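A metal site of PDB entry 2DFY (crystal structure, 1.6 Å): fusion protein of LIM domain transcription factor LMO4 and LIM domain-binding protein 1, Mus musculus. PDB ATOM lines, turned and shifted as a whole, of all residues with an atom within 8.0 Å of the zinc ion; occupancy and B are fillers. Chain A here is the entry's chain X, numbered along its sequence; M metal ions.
ND1 of His 27 binds the zinc ion (2.1 Å). The zinc ion is bound by the side-chain sulfur (SG) of Cys 30. SG of Cys 9 binds the zinc ion, at 2.3 Å. The side-chain sulfur (SG) of Cys 6 is bound to the zinc ion, at 2.4 Å. The zinc ion has four donor atoms within binding distance.
NE2 of His 27 lies within hydrogen-bond range of NH2 of Arg 29 (3.5 Å). A ring nitrogen (NE2) of His 27 lies within hydrogen-bond range of the backbone carbonyl oxygen of Lys 12 (3.4 Å). The side-chain sulfur (SG) of Cys 30 lies close to the guanidinium group (NH1) of Arg 29 (3.7 Å). The side-chain sulfur (SG) of Cys 9 sits close to the backbone NH (N) of Gly 11, at 3.3 Å. SG of Cys 6 sits close to N of Gly 8 (3.3 Å). The backbone carbonyl oxygen (O) of Gly 11 lies within hydrogen-bond range of the backbone NH (N) of Cys 6 (2.9 Å).
Four residues have an atom within 4 Å of the zinc ion: Cys 6, Cys 9, His 27 and Cys 30.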
ATOM      1  N   ARG A   5      -8.634  10.569  -0.081  1.00  0.00           N
ATOM      2  CA  ARG A   5      -9.507   9.818   0.804  1.00  0.00           C
ATOM      3  C   ARG A   5      -9.271  10.261   2.219  1.00  0.00           C
ATOM      4  O   ARG A   5      -8.151  10.620   2.580  1.00  0.00           O
ATOM      5  CB  ARG A   5      -9.361   8.296   0.670  1.00  0.00           C
ATOM      6  CG  ARG A   5     -10.066   7.724  -0.589  1.00  0.00           C
ATOM      7  CD  ARG A   5     -10.013   6.176  -0.599  1.00  0.00           C
ATOM      8  NE  ARG A   5     -10.590   5.662  -1.827  1.00  0.00           N
ATOM      9  CZ  ARG A   5     -11.893   5.523  -2.026  1.00  0.00           C
ATOM     10  NH1 ARG A   5     -12.739   5.857  -1.068  1.00  0.00           N
ATOM     11  NH2 ARG A   5     -12.335   5.034  -3.192  1.00  0.00           N
ATOM     12  N   CYS A   6     -10.347  10.266   2.992  1.00  0.00           N
ATOM     13  CA  CYS A   6     -10.329  10.650   4.394  1.00  0.00           C
ATOM     14  C   CYS A   6      -9.853   9.478   5.248  1.00  0.00           C
ATOM     15  O   CYS A   6     -10.365   8.368   5.114  1.00  0.00           O
ATOM     16  CB  CYS A   6     -11.739  11.010   4.804  1.00  0.00           C
ATOM     17  SG  CYS A   6     -11.929  11.442   6.530  1.00  0.00           S
ATOM     18  N   ALA A   7      -8.893   9.749   6.134  1.00  0.00           N
ATOM     19  CA  ALA A   7      -8.364   8.708   7.040  1.00  0.00           C
ATOM     20  C   ALA A   7      -9.401   8.313   8.110  1.00  0.00           C
ATOM     21  O   ALA A   7      -9.226   7.287   8.776  1.00  0.00           O
ATOM     22  CB  ALA A   7      -7.074   9.170   7.709  1.00  0.00           C
ATOM     23  N   GLY A   8     -10.404   9.173   8.350  1.00  0.00           N
ATOM     24  CA  GLY A   8     -11.397   8.919   9.384  1.00  0.00           C
ATOM     25  C   GLY A   8     -12.533   8.018   8.927  1.00  0.00           C
ATOM     26  O   GLY A   8     -13.023   7.199   9.700  1.00  0.00           O
ATOM     27  N   CYS A   9     -12.978   8.181   7.682  1.00  0.00           N
ATOM     28  CA  CYS A   9     -14.142   7.446   7.140  1.00  0.00           C
ATOM     29  C   CYS A   9     -13.885   6.666   5.859  1.00  0.00           C
ATOM     30  O   CYS A   9     -14.785   5.922   5.399  1.00  0.00           O
ATOM     31  CB  CYS A   9     -15.311   8.436   6.892  1.00  0.00           C
ATOM     32  SG  CYS A   9     -15.091   9.505   5.424  1.00  0.00           S
ATOM     33  N   GLY A  10     -12.696   6.817   5.256  1.00  0.00           N
ATOM     34  CA  GLY A  10     -12.318   6.161   4.005  1.00  0.00           C
ATOM     35  C   GLY A  10     -12.975   6.718   2.746  1.00  0.00           C
ATOM     36  O   GLY A  10     -12.688   6.247   1.630  1.00  0.00           O
ATOM     37  N   GLY A  11     -13.816   7.724   2.893  1.00  0.00           N
ATOM     38  CA  GLY A  11     -14.522   8.282   1.730  1.00  0.00           C
ATOM     39  C   GLY A  11     -13.700   9.319   0.979  1.00  0.00           C
ATOM     40  O   GLY A  11     -12.812   9.935   1.551  1.00  0.00           O
ATOM     41  N   LYS A  12     -14.012   9.548  -0.294  1.00  0.00           N
ATOM     42  CA  LYS A  12     -13.362  10.599  -1.049  1.00  0.00           C
ATOM     43  C   LYS A  12     -13.768  11.940  -0.478  1.00  0.00           C
ATOM     44  O   LYS A  12     -14.916  12.105  -0.049  1.00  0.00           O
ATOM     45  CB  LYS A  12     -13.754  10.539  -2.516  1.00  0.00           C
ATOM     46  CG  LYS A  12     -13.144   9.363  -3.282  1.00  0.00           C
ATOM     47  CD  LYS A  12     -13.473   9.440  -4.788  1.00  0.00           C
ATOM     48  CE  LYS A  12     -14.978   9.581  -5.070  1.00  0.00           C
ATOM     49  NZ  LYS A  12     -15.324   9.441  -6.529  1.00  0.00           N
ATOM     50  N   ILE A  13     -12.861  12.888  -0.469  1.00  0.00           N
ATOM     51  CA  ILE A  13     -13.151  14.184   0.117  1.00  0.00           C
ATOM     52  C   ILE A  13     -13.446  15.160  -1.036  1.00  0.00           C
ATOM     53  O   ILE A  13     -12.543  15.633  -1.731  1.00  0.00           O
ATOM     54  CB  ILE A  13     -12.020  14.739   1.021  1.00  0.00           C
ATOM     55  CG1 ILE A  13     -11.695  13.794   2.211  1.00  0.00           C
ATOM     56  CG2 ILE A  13     -12.435  16.091   1.589  1.00  0.00           C
ATOM     57  CD1 ILE A  13     -10.257  13.990   2.752  1.00  0.00           C
ATOM     58  N   ASP A  15     -15.305  17.992  -0.309  1.00  0.00           N
ATOM     59  CA  ASP A  15     -15.562  19.229   0.389  1.00  0.00           C
ATOM     60  C   ASP A  15     -14.639  20.340  -0.073  1.00  0.00           C
ATOM     61  O   ASP A  15     -13.459  20.095  -0.361  1.00  0.00           O
ATOM     62  CB  ASP A  15     -15.394  19.112   1.897  1.00  0.00           C
ATOM     63  CG  ASP A  15     -16.305  18.064   2.528  1.00  0.00           C
ATOM     64  OD1 ASP A  15     -17.121  17.423   1.833  1.00  0.00           O
ATOM     65  OD2 ASP A  15     -16.221  17.945   3.773  1.00  0.00           O
ATOM     66  N   TYR A  25      -5.280  13.147   4.997  1.00  0.00           N
ATOM     67  CA  TYR A  25      -6.357  14.147   4.727  1.00  0.00           C
ATOM     68  C   TYR A  25      -7.587  13.707   5.462  1.00  0.00           C
ATOM     69  O   TYR A  25      -7.804  12.499   5.641  1.00  0.00           O
ATOM     70  CB  TYR A  25      -6.658  14.204   3.233  1.00  0.00           C
ATOM     71  CG  TYR A  25      -5.481  14.692   2.405  1.00  0.00           C
ATOM     72  CD1 TYR A  25      -4.512  13.808   1.921  1.00  0.00           C
ATOM     73  CD2 TYR A  25      -5.317  16.054   2.128  1.00  0.00           C
ATOM     74  CE1 TYR A  25      -3.441  14.273   1.186  1.00  0.00           C
ATOM     75  CE2 TYR A  25      -4.282  16.499   1.385  1.00  0.00           C
ATOM     76  CZ  TYR A  25      -3.319  15.612   0.946  1.00  0.00           C
ATOM     77  OH  TYR A  25      -2.275  16.079   0.151  1.00  0.00           O
ATOM     78  N   TRP A  26      -8.452  14.669   5.823  1.00  0.00           N
ATOM     79  CA  TRP A  26      -9.644  14.400   6.598  1.00  0.00           C
ATOM     80  C   TRP A  26     -10.766  15.331   6.157  1.00  0.00           C
ATOM     81  O   TRP A  26     -10.504  16.501   5.983  1.00  0.00           O
ATOM     82  CB  TRP A  26      -9.388  14.694   8.084  1.00  0.00           C
ATOM     83  CG  TRP A  26      -8.177  14.023   8.674  1.00  0.00           C
ATOM     84  CD1 TRP A  26      -6.874  14.427   8.520  1.00  0.00           C
ATOM     85  CD2 TRP A  26      -8.137  12.874   9.528  1.00  0.00           C
ATOM     86  NE1 TRP A  26      -6.023  13.588   9.207  1.00  0.00           N
ATOM     87  CE2 TRP A  26      -6.777  12.619   9.823  1.00  0.00           C
ATOM     88  CE3 TRP A  26      -9.117  12.011  10.052  1.00  0.00           C
ATOM     89  CZ2 TRP A  26      -6.388  11.558  10.622  1.00  0.00           C
ATOM     90  CZ3 TRP A  26      -8.705  10.959  10.854  1.00  0.00           C
ATOM     91  CH2 TRP A  26      -7.343  10.741  11.105  1.00  0.00           C
ATOM     92  N   HIS A  27     -11.989  14.835   6.101  1.00  0.00           N
ATOM     93  CA  HIS A  27     -13.168  15.714   6.293  1.00  0.00           C
ATOM     94  C   HIS A  27     -13.001  16.288   7.685  1.00  0.00           C
ATOM     95  O   HIS A  27     -12.606  15.544   8.608  1.00  0.00           O
ATOM     96  CB  HIS A  27     -14.470  14.890   6.283  1.00  0.00           C
ATOM     97  CG  HIS A  27     -14.791  14.205   4.992  1.00  0.00           C
ATOM     98  ND1 HIS A  27     -14.709  12.829   4.850  1.00  0.00           N
ATOM     99  CD2 HIS A  27     -15.321  14.671   3.827  1.00  0.00           C
ATOM    100  CE1 HIS A  27     -15.128  12.482   3.641  1.00  0.00           C
ATOM    101  NE2 HIS A  27     -15.502  13.586   2.986  1.00  0.00           N
ATOM    102  N   SER A  28     -13.251  17.590   7.906  1.00  0.00           N
ATOM    103  CA  SER A  28     -13.083  18.146   9.251  1.00  0.00           C
ATOM    104  C   SER A  28     -13.935  17.334  10.240  1.00  0.00           C
ATOM    105  O   SER A  28     -13.468  17.058  11.338  1.00  0.00           O
ATOM    106  CB  SER A  28     -13.422  19.643   9.355  1.00  0.00           C
ATOM    107  OG  SER A  28     -13.234  20.055  10.671  1.00  0.00           O
ATOM    108  N   ARG A  29     -15.159  16.936   9.848  1.00  0.00           N
ATOM    109  CA  ARG A  29     -16.046  16.227  10.807  1.00  0.00           C
ATOM    110  C   ARG A  29     -15.501  14.860  11.265  1.00  0.00           C
ATOM    111  O   ARG A  29     -16.012  14.282  12.236  1.00  0.00           O
ATOM    112  CB  ARG A  29     -17.416  16.029  10.146  1.00  0.00           C
ATOM    113  CG  ARG A  29     -17.413  15.278   8.838  1.00  0.00           C
ATOM    114  CD  ARG A  29     -18.725  15.234   8.068  1.00  0.00           C
ATOM    115  NE  ARG A  29     -18.531  14.762   6.689  1.00  0.00           N
ATOM    116  CZ  ARG A  29     -18.482  13.494   6.279  1.00  0.00           C
ATOM    117  NH1 ARG A  29     -18.649  12.488   7.142  1.00  0.00           N
ATOM    118  NH2 ARG A  29     -18.284  13.230   5.020  1.00  0.00           N
ATOM    119  N   CYS A  30     -14.548  14.328  10.508  1.00  0.00           N
ATOM    120  CA  CYS A  30     -13.967  13.006  10.759  1.00  0.00           C
ATOM    121  C   CYS A  30     -12.745  12.997  11.641  1.00  0.00           C
ATOM    122  O   CYS A  30     -12.242  11.919  12.047  1.00  0.00           O
ATOM    123  CB  CYS A  30     -13.663  12.347   9.416  1.00  0.00           C
ATOM    124  SG  CYS A  30     -15.182  12.005   8.435  1.00  0.00           S
ATOM    125  N   LEU A  31     -12.184  14.192  11.875  1.00  0.00           N
ATOM    126  CA  LEU A  31     -11.002  14.288  12.760  1.00  0.00           C
ATOM    127  C   LEU A  31     -11.460  14.775  14.129  1.00  0.00           C
ATOM    128  O   LEU A  31     -11.622  15.981  14.389  1.00  0.00           O
ATOM    129  CB  LEU A  31      -9.911  15.190  12.157  1.00  0.00           C
ATOM    130  CG  LEU A  31      -8.625  15.346  12.957  1.00  0.00           C
ATOM    131  CD1 LEU A  31      -7.996  13.987  13.245  1.00  0.00           C
ATOM    132  CD2 LEU A  31      -7.625  16.358  12.354  1.00  0.00           C
HETATM  133 ZN    ZN M   1     -14.280  11.459   6.409  1.00  0.00          ZN
